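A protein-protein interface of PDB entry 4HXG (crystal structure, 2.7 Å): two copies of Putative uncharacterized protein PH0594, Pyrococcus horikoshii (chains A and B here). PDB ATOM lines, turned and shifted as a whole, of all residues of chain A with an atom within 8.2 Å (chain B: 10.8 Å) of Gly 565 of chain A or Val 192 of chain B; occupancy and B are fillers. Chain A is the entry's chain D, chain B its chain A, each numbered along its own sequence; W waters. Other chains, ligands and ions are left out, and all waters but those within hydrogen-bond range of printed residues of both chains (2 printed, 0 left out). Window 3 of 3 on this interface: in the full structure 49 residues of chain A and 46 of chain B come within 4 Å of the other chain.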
ATOM      1  N   ALA A 531      -4.713  12.628  -8.746  1.00  0.00           N
ATOM      2  CA  ALA A 531      -3.719  12.756  -9.813  1.00  0.00           C
ATOM      3  C   ALA A 531      -3.939  13.944 -10.750  1.00  0.00           C
ATOM      4  O   ALA A 531      -2.976  14.526 -11.257  1.00  0.00           O
ATOM      5  CB  ALA A 531      -3.636  11.467 -10.609  1.00  0.00           C
ATOM      6  N   VAL A 534      -1.636  17.043 -10.044  1.00  0.00           N
ATOM      7  CA  VAL A 534      -0.192  17.178 -10.158  1.00  0.00           C
ATOM      8  C   VAL A 534       0.162  18.198 -11.245  1.00  0.00           C
ATOM      9  O   VAL A 534      -0.239  18.044 -12.399  1.00  0.00           O
ATOM     10  CB  VAL A 534       0.431  15.810 -10.525  1.00  0.00           C
ATOM     11  CG1 VAL A 534       1.920  15.946 -10.788  1.00  0.00           C
ATOM     12  CG2 VAL A 534       0.159  14.791  -9.431  1.00  0.00           C
ATOM     13  N   TYR A 558       1.476   6.067 -12.754  1.00  0.00           N
ATOM     14  CA  TYR A 558       2.098   6.514 -13.994  1.00  0.00           C
ATOM     15  C   TYR A 558       1.100   6.550 -15.137  1.00  0.00           C
ATOM     16  O   TYR A 558       0.950   7.571 -15.808  1.00  0.00           O
ATOM     17  CB  TYR A 558       3.251   5.589 -14.371  1.00  0.00           C
ATOM     18  CG  TYR A 558       3.800   5.836 -15.750  1.00  0.00           C
ATOM     19  CD1 TYR A 558       4.737   6.828 -15.976  1.00  0.00           C
ATOM     20  CD2 TYR A 558       3.384   5.069 -16.830  1.00  0.00           C
ATOM     21  CE1 TYR A 558       5.247   7.052 -17.243  1.00  0.00           C
ATOM     22  CE2 TYR A 558       3.892   5.284 -18.109  1.00  0.00           C
ATOM     23  CZ  TYR A 558       4.818   6.276 -18.306  1.00  0.00           C
ATOM     24  OH  TYR A 558       5.319   6.500 -19.565  1.00  0.00           O
ATOM     25  N   HIS A 559       0.427   5.424 -15.355  1.00  0.00           N
ATOM     26  CA  HIS A 559      -0.532   5.305 -16.440  1.00  0.00           C
ATOM     27  C   HIS A 559      -1.606   6.370 -16.312  1.00  0.00           C
ATOM     28  O   HIS A 559      -1.928   7.070 -17.273  1.00  0.00           O
ATOM     29  CB  HIS A 559      -1.151   3.912 -16.448  1.00  0.00           C
ATOM     30  CG  HIS A 559      -0.309   2.889 -17.143  1.00  0.00           C
ATOM     31  ND1 HIS A 559      -0.486   1.532 -16.976  1.00  0.00           N
ATOM     32  CD2 HIS A 559       0.713   3.031 -18.019  1.00  0.00           C
ATOM     33  CE1 HIS A 559       0.395   0.883 -17.715  1.00  0.00           C
ATOM     34  NE2 HIS A 559       1.135   1.769 -18.359  1.00  0.00           N
ATOM     35  N   VAL A 560      -2.157   6.500 -15.115  1.00  0.00           N
ATOM     36  CA  VAL A 560      -3.179   7.502 -14.900  1.00  0.00           C
ATOM     37  C   VAL A 560      -2.628   8.882 -15.283  1.00  0.00           C
ATOM     38  O   VAL A 560      -3.166   9.541 -16.169  1.00  0.00           O
ATOM     39  CB  VAL A 560      -3.719   7.449 -13.448  1.00  0.00           C
ATOM     40  CG1 VAL A 560      -4.400   8.755 -13.061  1.00  0.00           C
ATOM     41  CG2 VAL A 560      -4.688   6.285 -13.292  1.00  0.00           C
ATOM     42  N   LEU A 561      -1.528   9.289 -14.659  1.00  0.00           N
ATOM     43  CA  LEU A 561      -0.920  10.584 -14.949  1.00  0.00           C
ATOM     44  C   LEU A 561      -0.744  10.838 -16.447  1.00  0.00           C
ATOM     45  O   LEU A 561      -0.970  11.953 -16.927  1.00  0.00           O
ATOM     46  CB  LEU A 561       0.426  10.702 -14.247  1.00  0.00           C
ATOM     47  CG  LEU A 561       0.277  10.854 -12.743  1.00  0.00           C
ATOM     48  CD1 LEU A 561       1.591  10.545 -12.030  1.00  0.00           C
ATOM     49  CD2 LEU A 561      -0.229  12.256 -12.439  1.00  0.00           C
ATOM     50  N   LYS A 562      -0.332   9.813 -17.184  1.00  0.00           N
ATOM     51  CA  LYS A 562      -0.191   9.956 -18.623  1.00  0.00           C
ATOM     52  C   LYS A 562      -1.559  10.170 -19.262  1.00  0.00           C
ATOM     53  O   LYS A 562      -1.697  10.980 -20.170  1.00  0.00           O
ATOM     54  CB  LYS A 562       0.495   8.734 -19.235  1.00  0.00           C
ATOM     55  CG  LYS A 562       1.963   8.564 -18.856  1.00  0.00           C
ATOM     56  CD  LYS A 562       2.833   9.707 -19.374  1.00  0.00           C
ATOM     57  CE  LYS A 562       2.953   9.691 -20.889  1.00  0.00           C
ATOM     58  NZ  LYS A 562       3.909  10.729 -21.374  1.00  0.00           N
ATOM     59  N   ASP A 563      -2.566   9.442 -18.787  1.00  0.00           N
ATOM     60  CA  ASP A 563      -3.915   9.559 -19.336  1.00  0.00           C
ATOM     61  C   ASP A 563      -4.451  10.972 -19.122  1.00  0.00           C
ATOM     62  O   ASP A 563      -5.298  11.443 -19.884  1.00  0.00           O
ATOM     63  CB  ASP A 563      -4.856   8.528 -18.709  1.00  0.00           C
ATOM     64  CG  ASP A 563      -6.002   8.143 -19.632  1.00  0.00           C
ATOM     65  OD1 ASP A 563      -5.835   8.297 -20.860  1.00  0.00           O
ATOM     66  OD2 ASP A 563      -7.062   7.683 -19.143  1.00  0.00           O
ATOM     67  N   LEU A 564      -3.939  11.643 -18.091  1.00  0.00           N
ATOM     68  CA  LEU A 564      -4.294  13.035 -17.788  1.00  0.00           C
ATOM     69  C   LEU A 564      -3.368  14.063 -18.444  1.00  0.00           C
ATOM     70  O   LEU A 564      -3.446  15.251 -18.147  1.00  0.00           O
ATOM     71  CB  LEU A 564      -4.373  13.268 -16.276  1.00  0.00           C
ATOM     72  CG  LEU A 564      -5.399  12.388 -15.556  1.00  0.00           C
ATOM     73  CD1 LEU A 564      -5.301  12.543 -14.047  1.00  0.00           C
ATOM     74  CD2 LEU A 564      -6.804  12.693 -16.040  1.00  0.00           C
ATOM     75  N   GLY A 565      -2.452  13.591 -19.281  1.00  0.00           N
ATOM     76  CA  GLY A 565      -1.587  14.474 -20.048  1.00  0.00           C
ATOM     77  C   GLY A 565      -0.417  15.067 -19.283  1.00  0.00           C
ATOM     78  O   GLY A 565       0.204  16.019 -19.747  1.00  0.00           O
ATOM     79  N   LYS A 566      -0.118  14.500 -18.116  1.00  0.00           N
ATOM     80  CA  LYS A 566       0.966  14.971 -17.255  1.00  0.00           C
ATOM     81  C   LYS A 566       2.365  14.570 -17.747  1.00  0.00           C
ATOM     82  O   LYS A 566       2.518  13.588 -18.480  1.00  0.00           O
ATOM     83  CB  LYS A 566       0.757  14.425 -15.846  1.00  0.00           C
ATOM     84  CG  LYS A 566      -0.664  14.579 -15.332  1.00  0.00           C
ATOM     85  CD  LYS A 566      -0.983  16.030 -15.030  1.00  0.00           C
ATOM     86  CE  LYS A 566      -2.277  16.160 -14.256  1.00  0.00           C
ATOM     87  NZ  LYS A 566      -2.602  17.589 -14.028  1.00  0.00           N
ATOM     88  N   GLU A 567       3.389  15.310 -17.327  1.00  0.00           N
ATOM     89  CA  GLU A 567       4.752  14.898 -17.634  1.00  0.00           C
ATOM     90  C   GLU A 567       5.293  14.029 -16.514  1.00  0.00           C
ATOM     91  O   GLU A 567       5.537  14.497 -15.400  1.00  0.00           O
ATOM     92  CB  GLU A 567       5.684  16.090 -17.820  1.00  0.00           C
ATOM     93  CG  GLU A 567       7.137  15.668 -18.030  1.00  0.00           C
ATOM     94  CD  GLU A 567       8.104  16.822 -17.921  1.00  0.00           C
ATOM     95  OE1 GLU A 567       9.328  16.581 -17.993  1.00  0.00           O
ATOM     96  OE2 GLU A 567       7.641  17.972 -17.759  1.00  0.00           O
ATOM     97  N   VAL A 568       5.496  12.758 -16.833  1.00  0.00           N
ATOM     98  CA  VAL A 568       5.929  11.779 -15.858  1.00  0.00           C
ATOM     99  C   VAL A 568       6.720  10.700 -16.594  1.00  0.00           C
ATOM    100  O   VAL A 568       6.477  10.450 -17.779  1.00  0.00           O
ATOM    101  CB  VAL A 568       4.713  11.182 -15.097  1.00  0.00           C
ATOM    102  CG1 VAL A 568       3.815  10.393 -16.043  1.00  0.00           C
ATOM    103  CG2 VAL A 568       5.165  10.328 -13.926  1.00  0.00           C
ATOM    104  N   ASP B 135       8.524   6.530 -21.194  1.00  0.00           N
ATOM    105  CA  ASP B 135       7.886   7.843 -21.291  1.00  0.00           C
ATOM    106  C   ASP B 135       6.488   7.883 -21.936  1.00  0.00           C
ATOM    107  O   ASP B 135       5.859   8.939 -21.982  1.00  0.00           O
ATOM    108  CB  ASP B 135       8.819   8.855 -21.964  1.00  0.00           C
ATOM    109  CG  ASP B 135       9.556   8.278 -23.156  1.00  0.00           C
ATOM    110  OD1 ASP B 135      10.504   8.942 -23.639  1.00  0.00           O
ATOM    111  OD2 ASP B 135       9.204   7.165 -23.601  1.00  0.00           O
ATOM    112  N   ASP B 136       5.998   6.739 -22.404  1.00  0.00           N
ATOM    113  CA  ASP B 136       4.742   6.673 -23.166  1.00  0.00           C
ATOM    114  C   ASP B 136       3.794   5.676 -22.491  1.00  0.00           C
ATOM    115  O   ASP B 136       4.058   5.251 -21.363  1.00  0.00           O
ATOM    116  CB  ASP B 136       4.999   6.278 -24.630  1.00  0.00           C
ATOM    117  CG  ASP B 136       3.945   6.834 -25.593  1.00  0.00           C
ATOM    118  OD1 ASP B 136       2.894   7.320 -25.128  1.00  0.00           O
ATOM    119  OD2 ASP B 136       4.164   6.780 -26.822  1.00  0.00           O
ATOM    120  N   VAL B 137       2.669   5.356 -23.135  1.00  0.00           N
ATOM    121  CA  VAL B 137       1.742   4.349 -22.603  1.00  0.00           C
ATOM    122  C   VAL B 137       1.295   3.350 -23.663  1.00  0.00           C
ATOM    123  O   VAL B 137       1.176   3.701 -24.840  1.00  0.00           O
ATOM    124  CB  VAL B 137       0.479   4.984 -22.027  1.00  0.00           C
ATOM    125  CG1 VAL B 137       0.828   5.901 -20.887  1.00  0.00           C
ATOM    126  CG2 VAL B 137      -0.247   5.732 -23.111  1.00  0.00           C
ATOM    127  N   PRO B 138       1.043   2.097 -23.251  1.00  0.00           N
ATOM    128  CA  PRO B 138       1.258   1.594 -21.886  1.00  0.00           C
ATOM    129  C   PRO B 138       2.706   1.178 -21.654  1.00  0.00           C
ATOM    130  O   PRO B 138       3.526   1.277 -22.561  1.00  0.00           O
ATOM    131  CB  PRO B 138       0.358   0.363 -21.833  1.00  0.00           C
ATOM    132  CG  PRO B 138       0.346  -0.135 -23.231  1.00  0.00           C
ATOM    133  CD  PRO B 138       0.404   1.086 -24.113  1.00  0.00           C
ATOM    134  N   PRO B 188      -1.023   4.289 -35.194  1.00  0.00           N
ATOM    135  CA  PRO B 188      -1.977   4.732 -34.173  1.00  0.00           C
ATOM    136  C   PRO B 188      -2.042   6.254 -34.107  1.00  0.00           C
ATOM    137  O   PRO B 188      -1.021   6.907 -34.312  1.00  0.00           O
ATOM    138  CB  PRO B 188      -1.381   4.164 -32.882  1.00  0.00           C
ATOM    139  CG  PRO B 188      -0.666   2.934 -33.326  1.00  0.00           C
ATOM    140  CD  PRO B 188      -0.093   3.269 -34.679  1.00  0.00           C
ATOM    141  N   HIS B 189      -3.221   6.805 -33.832  1.00  0.00           N
ATOM    142  CA  HIS B 189      -3.389   8.254 -33.768  1.00  0.00           C
ATOM    143  C   HIS B 189      -3.164   8.765 -32.347  1.00  0.00           C
ATOM    144  O   HIS B 189      -3.582   8.132 -31.378  1.00  0.00           O
ATOM    145  CB  HIS B 189      -4.780   8.661 -34.263  1.00  0.00           C
ATOM    146  CG  HIS B 189      -5.025  10.138 -34.230  1.00  0.00           C
ATOM    147  ND1 HIS B 189      -4.589  10.990 -35.222  1.00  0.00           N
ATOM    148  CD2 HIS B 189      -5.659  10.917 -33.321  1.00  0.00           C
ATOM    149  CE1 HIS B 189      -4.943  12.227 -34.926  1.00  0.00           C
ATOM    150  NE2 HIS B 189      -5.594  12.211 -33.778  1.00  0.00           N
ATOM    151  N   ARG B 190      -2.500   9.908 -32.228  1.00  0.00           N
ATOM    152  CA  ARG B 190      -2.170  10.451 -30.916  1.00  0.00           C
ATOM    153  C   ARG B 190      -2.960  11.711 -30.599  1.00  0.00           C
ATOM    154  O   ARG B 190      -2.877  12.706 -31.319  1.00  0.00           O
ATOM    155  CB  ARG B 190      -0.667  10.743 -30.815  1.00  0.00           C
ATOM    156  CG  ARG B 190      -0.239  11.345 -29.478  1.00  0.00           C
ATOM    157  CD  ARG B 190       1.270  11.584 -29.428  1.00  0.00           C
ATOM    158  NE  ARG B 190       2.027  10.369 -29.728  1.00  0.00           N
ATOM    159  CZ  ARG B 190       2.375   9.459 -28.822  1.00  0.00           C
ATOM    160  NH1 ARG B 190       2.041   9.627 -27.547  1.00  0.00           N
ATOM    161  NH2 ARG B 190       3.058   8.377 -29.185  1.00  0.00           N
ATOM    162  N   ASP B 191      -3.727  11.668 -29.517  1.00  0.00           N
ATOM    163  CA  ASP B 191      -4.359  12.877 -29.013  1.00  0.00           C
ATOM    164  C   ASP B 191      -3.642  13.298 -27.737  1.00  0.00           C
ATOM    165  O   ASP B 191      -2.822  14.219 -27.741  1.00  0.00           O
ATOM    166  CB  ASP B 191      -5.845  12.637 -28.740  1.00  0.00           C
ATOM    167  CG  ASP B 191      -6.688  12.689 -30.004  1.00  0.00           C
ATOM    168  OD1 ASP B 191      -6.437  13.566 -30.863  1.00  0.00           O
ATOM    169  OD2 ASP B 191      -7.604  11.849 -30.136  1.00  0.00           O
ATOM    170  N   VAL B 192      -3.923  12.588 -26.656  1.00  0.00           N
ATOM    171  CA  VAL B 192      -3.194  12.771 -25.416  1.00  0.00           C
ATOM    172  C   VAL B 192      -2.240  11.596 -25.333  1.00  0.00           C
ATOM    173  O   VAL B 192      -1.020  11.749 -25.314  1.00  0.00           O
ATOM    174  CB  VAL B 192      -4.129  12.768 -24.203  1.00  0.00           C
ATOM    175  CG1 VAL B 192      -3.316  12.923 -22.911  1.00  0.00           C
ATOM    176  CG2 VAL B 192      -5.193  13.857 -24.335  1.00  0.00           C
ATOM    177  N   ILE B 193      -2.835  10.413 -25.279  1.00  0.00           N
ATOM    178  CA  ILE B 193      -2.122   9.160 -25.377  1.00  0.00           C
ATOM    179  C   ILE B 193      -2.578   8.561 -26.693  1.00  0.00           C
ATOM    180  O   ILE B 193      -3.634   8.931 -27.205  1.00  0.00           O
ATOM    181  CB  ILE B 193      -2.510   8.214 -24.238  1.00  0.00           C
ATOM    182  CG1 ILE B 193      -4.014   7.946 -24.267  1.00  0.00           C
ATOM    183  CG2 ILE B 193      -2.126   8.807 -22.896  1.00  0.00           C
ATOM    184  CD1 ILE B 193      -4.463   6.886 -23.284  1.00  0.00           C
ATOM    185  N   PRO B 194      -1.761   7.680 -27.285  1.00  0.00           N
ATOM    186  CA  PRO B 194      -2.181   7.045 -28.539  1.00  0.00           C
ATOM    187  C   PRO B 194      -3.518   6.328 -28.357  1.00  0.00           C
ATOM    188  O   PRO B 194      -3.746   5.712 -27.308  1.00  0.00           O
ATOM    189  CB  PRO B 194      -1.069   6.025 -28.804  1.00  0.00           C
ATOM    190  CG  PRO B 194       0.108   6.550 -28.074  1.00  0.00           C
ATOM    191  CD  PRO B 194      -0.440   7.207 -26.842  1.00  0.00           C
ATOM    192  N   ARG B 195      -4.389   6.382 -29.360  1.00  0.00           N
ATOM    193  CA  ARG B 195      -5.668   5.714 -29.223  1.00  0.00           C
ATOM    194  C   ARG B 195      -5.527   4.411 -29.970  1.00  0.00           C
ATOM    195  O   ARG B 195      -5.571   4.379 -31.196  1.00  0.00           O
ATOM    196  CB  ARG B 195      -6.770   6.551 -29.872  1.00  0.00           C
ATOM    197  CG  ARG B 195      -6.645   8.047 -29.646  1.00  0.00           C
ATOM    198  CD  ARG B 195      -6.927   8.404 -28.203  1.00  0.00           C
ATOM    199  NE  ARG B 195      -8.255   7.957 -27.800  1.00  0.00           N
ATOM    200  CZ  ARG B 195      -9.376   8.638 -28.036  1.00  0.00           C
ATOM    201  NH1 ARG B 195      -9.330   9.805 -28.673  1.00  0.00           N
ATOM    202  NH2 ARG B 195     -10.545   8.154 -27.638  1.00  0.00           N
ATOM    203  N   TYR B 196      -5.419   3.326 -29.213  1.00  0.00           N
ATOM    204  CA  TYR B 196      -5.137   2.026 -29.795  1.00  0.00           C
ATOM    205  C   TYR B 196      -6.443   1.303 -30.062  1.00  0.00           C
ATOM    206  O   TYR B 196      -7.352   1.323 -29.230  1.00  0.00           O
ATOM    207  CB  TYR B 196      -4.264   1.175 -28.872  1.00  0.00           C
ATOM    208  CG  TYR B 196      -2.863   1.689 -28.639  1.00  0.00           C
ATOM    209  CD1 TYR B 196      -2.460   2.097 -27.376  1.00  0.00           C
ATOM    210  CD2 TYR B 196      -1.935   1.742 -29.670  1.00  0.00           C
ATOM    211  CE1 TYR B 196      -1.184   2.555 -27.143  1.00  0.00           C
ATOM    212  CE2 TYR B 196      -0.647   2.204 -29.446  1.00  0.00           C
ATOM    213  CZ  TYR B 196      -0.280   2.608 -28.176  1.00  0.00           C
ATOM    214  OH  TYR B 196       0.994   3.071 -27.925  1.00  0.00           O
ATOM    215  N   TYR B 199      -8.405   4.761 -33.418  1.00  0.00           N
ATOM    216  CA  TYR B 199      -8.100   5.638 -34.546  1.00  0.00           C
ATOM    217  C   TYR B 199      -6.683   5.453 -35.115  1.00  0.00           C
ATOM    218  O   TYR B 199      -5.725   5.224 -34.371  1.00  0.00           O
ATOM    219  CB  TYR B 199      -8.325   7.104 -34.163  1.00  0.00           C
ATOM    220  CG  TYR B 199      -9.734   7.436 -33.715  1.00  0.00           C
ATOM    221  CD1 TYR B 199     -10.009   7.737 -32.385  1.00  0.00           C
ATOM    222  CD2 TYR B 199     -10.786   7.464 -34.622  1.00  0.00           C
ATOM    223  CE1 TYR B 199     -11.292   8.051 -31.971  1.00  0.00           C
ATOM    224  CE2 TYR B 199     -12.075   7.776 -34.215  1.00  0.00           C
ATOM    225  CZ  TYR B 199     -12.323   8.067 -32.889  1.00  0.00           C
ATOM    226  OH  TYR B 199     -13.605   8.377 -32.477  1.00  0.00           O
ATOM    227  N   LYS B 216      -7.274  10.150 -38.625  1.00  0.00           N
ATOM    228  CA  LYS B 216      -8.178   9.797 -37.533  1.00  0.00           C
ATOM    229  C   LYS B 216      -9.342   8.907 -37.956  1.00  0.00           C
ATOM    230  O   LYS B 216     -10.496   9.225 -37.688  1.00  0.00           O
ATOM    231  CB  LYS B 216      -8.688  11.037 -36.798  1.00  0.00           C
ATOM    232  CG  LYS B 216      -9.175  10.732 -35.388  1.00  0.00           C
ATOM    233  CD  LYS B 216      -9.392  11.998 -34.583  1.00  0.00           C
ATOM    234  CE  LYS B 216      -9.942  11.683 -33.201  1.00  0.00           C
ATOM    235  NZ  LYS B 216     -10.064  12.903 -32.356  1.00  0.00           N
ATOM    236  N   TYR B 498      -8.071  -1.060 -15.073  1.00  0.00           N
ATOM    237  CA  TYR B 498      -7.907   0.194 -15.794  1.00  0.00           C
ATOM    238  C   TYR B 498      -6.491   0.762 -15.676  1.00  0.00           C
ATOM    239  O   TYR B 498      -5.866   1.100 -16.677  1.00  0.00           O
ATOM    240  CB  TYR B 498      -8.920   1.225 -15.296  1.00  0.00           C
ATOM    241  CG  TYR B 498      -8.558   2.668 -15.605  1.00  0.00           C
ATOM    242  CD1 TYR B 498      -8.640   3.169 -16.902  1.00  0.00           C
ATOM    243  CD2 TYR B 498      -8.154   3.530 -14.600  1.00  0.00           C
ATOM    244  CE1 TYR B 498      -8.320   4.484 -17.186  1.00  0.00           C
ATOM    245  CE2 TYR B 498      -7.832   4.855 -14.877  1.00  0.00           C
ATOM    246  CZ  TYR B 498      -7.919   5.328 -16.173  1.00  0.00           C
ATOM    247  OH  TYR B 498      -7.599   6.642 -16.454  1.00  0.00           O
ATOM    248  N   LEU B 505      -6.372   1.557 -20.045  1.00  0.00           N
ATOM    249  CA  LEU B 505      -6.679   2.988 -20.178  1.00  0.00           C
ATOM    250  C   LEU B 505      -7.851   3.308 -21.118  1.00  0.00           C
ATOM    251  O   LEU B 505      -8.651   4.204 -20.833  1.00  0.00           O
ATOM    252  CB  LEU B 505      -5.437   3.790 -20.589  1.00  0.00           C
ATOM    253  CG  LEU B 505      -4.333   4.027 -19.552  1.00  0.00           C
ATOM    254  CD1 LEU B 505      -3.238   4.901 -20.122  1.00  0.00           C
ATOM    255  CD2 LEU B 505      -4.874   4.656 -18.283  1.00  0.00           C
ATOM    256  N   LYS B 509     -12.620   2.064 -20.069  1.00  0.00           N
ATOM    257  CA  LYS B 509     -13.514   3.214 -20.135  1.00  0.00           C
ATOM    258  C   LYS B 509     -14.806   2.891 -20.872  1.00  0.00           C
ATOM    259  O   LYS B 509     -15.869   3.390 -20.522  1.00  0.00           O
ATOM    260  CB  LYS B 509     -12.823   4.409 -20.786  1.00  0.00           C
ATOM    261  CG  LYS B 509     -12.069   5.286 -19.810  1.00  0.00           C
ATOM    262  CD  LYS B 509     -11.154   6.212 -20.563  1.00  0.00           C
ATOM    263  CE  LYS B 509     -10.612   7.308 -19.695  1.00  0.00           C
ATOM    264  NZ  LYS B 509      -9.830   8.208 -20.566  1.00  0.00           N
ATOM    265  N   LEU B 517     -11.777   7.168 -11.745  1.00  0.00           N
ATOM    266  CA  LEU B 517     -11.405   7.582 -10.405  1.00  0.00           C
ATOM    267  C   LEU B 517     -12.648   7.945  -9.610  1.00  0.00           C
ATOM    268  O   LEU B 517     -12.603   8.174  -8.407  1.00  0.00           O
ATOM    269  CB  LEU B 517     -10.415   8.744 -10.475  1.00  0.00           C
ATOM    270  CG  LEU B 517      -9.052   8.314 -11.038  1.00  0.00           C
ATOM    271  CD1 LEU B 517      -8.093   9.482 -11.158  1.00  0.00           C
ATOM    272  CD2 LEU B 517      -8.459   7.231 -10.165  1.00  0.00           C
HETATM  273  O   HOH W   1      -3.350   1.181 -18.591  1.00  0.00           O
HETATM  274  O   HOH W   2      -8.081   9.173 -16.181  1.00  0.00           O
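OH of Tyr 558 of chain A sits close to O of Asp 135 of chain B (3.5 Å). O of Asp 135 of chain B lies within hydrogen-bond range of NZ of Lys 562 of chain A (2.7 Å). OH of Tyr 558 of chain A lies within hydrogen-bond range of O of Asp 136 of chain B (2.5 Å). The side-chain carboxylate (OD2) of Asp 563 of chain A is in hydrogen-bond range of the side-chain hydroxyl (OH) of Tyr 498 of chain B, at 2.9 Å. The side-chain carboxylate (OD2) of Asp 563 of chain A is in salt-bridge range of the side-chain amino group (NZ) of Lys 509 of chain B (3.2 Å).
OD2 of Asp 136 of chain B lies within salt-bridge range of NH2 of Arg 190 of chain B (3.1 Å). O of Val 137 of chain B sits at hydrogen-bond distance from OH of Tyr 196 of chain B, at 3.2 Å. O of Tyr 498 of chain B lies within hydrogen-bond range of N of Leu 505 of chain B.
Among the printed residues, pairs that only touch across the chains: His 559 of chain A with Pro 138 of chain B, His 559 of chain A with Leu 505 of chain B, Val 560 of chain A with Tyr 498 of chain B, Lys 562 of chain A with Val 137 of chain B, Lys 562 of chain A with Val 192 of chain B, Lys 562 of chain A with Ile 193 of chain B, Asp 563 of chain A with Val 192 of chain B, Asp 563 of chain A with Ile 193 of chain B, Asp 563 of chain A with Leu 505 of chain B and Gly 565 of chain A with Val 192 of chain B.
Of chain A, only Lys 562, Asp 563 and Gly 565 come within 4 Å of Val 192 of chain B. No residue of chain B comes within 4 Å of Leu 564 of chain A. Of the printed residues of chain A, Asp 136 of chain B touches Tyr 558. Printed residues of chain A within 4 Å of Tyr 498 of chain B: Val 560 and Asp 563. Arg 195 of chain B touches none of the printed residues of chain A. Ala 531 of chain A touches none of the printed residues of chain B. The nearest residue of chain B that does not touch Gly 565 of chain A is Ile 193 of chain B (6.0 Å).
Of the 13 printed residues of chain A, 6 touch a printed residue of chain B. Printed residues of chain B that touch a printed residue of chain A: Asp 135, Asp 136, Val 137, Pro 138, Val 192, Ile 193, Tyr 498, Leu 505 and Lys 509. Hydrophobic or aromatic side chains of chain B within 4 Å of the printed part of chain A: Val 137, Pro 138, Val 192, Ile 193, Tyr 498 and Leu 505. Among the printed residues, 15 pairs touch across the chains. Among the printed residues, Asp or Glu carboxylates within 4 Å of a Lys or Arg side-chain nitrogen of the other chain: Asp 563 of chain A with Lys 509 of chain B (3.2 Å).
No position is printed for both chains.
Water W2 lies within hydrogen-bond range of OH of Tyr 498 of chain B (2.6 Å) and OD2 of Asp 563 of chain A (3.5 Å). Water W1 lies within hydrogen-bond range of the backbone carbonyl oxygen (O) of Tyr 498 of chain B (3.2 Å), a ring nitrogen (ND1) of His 559 of chain A (3.3 Å) and the backbone NH (N) of Leu 505 of chain B (3.4 Å).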
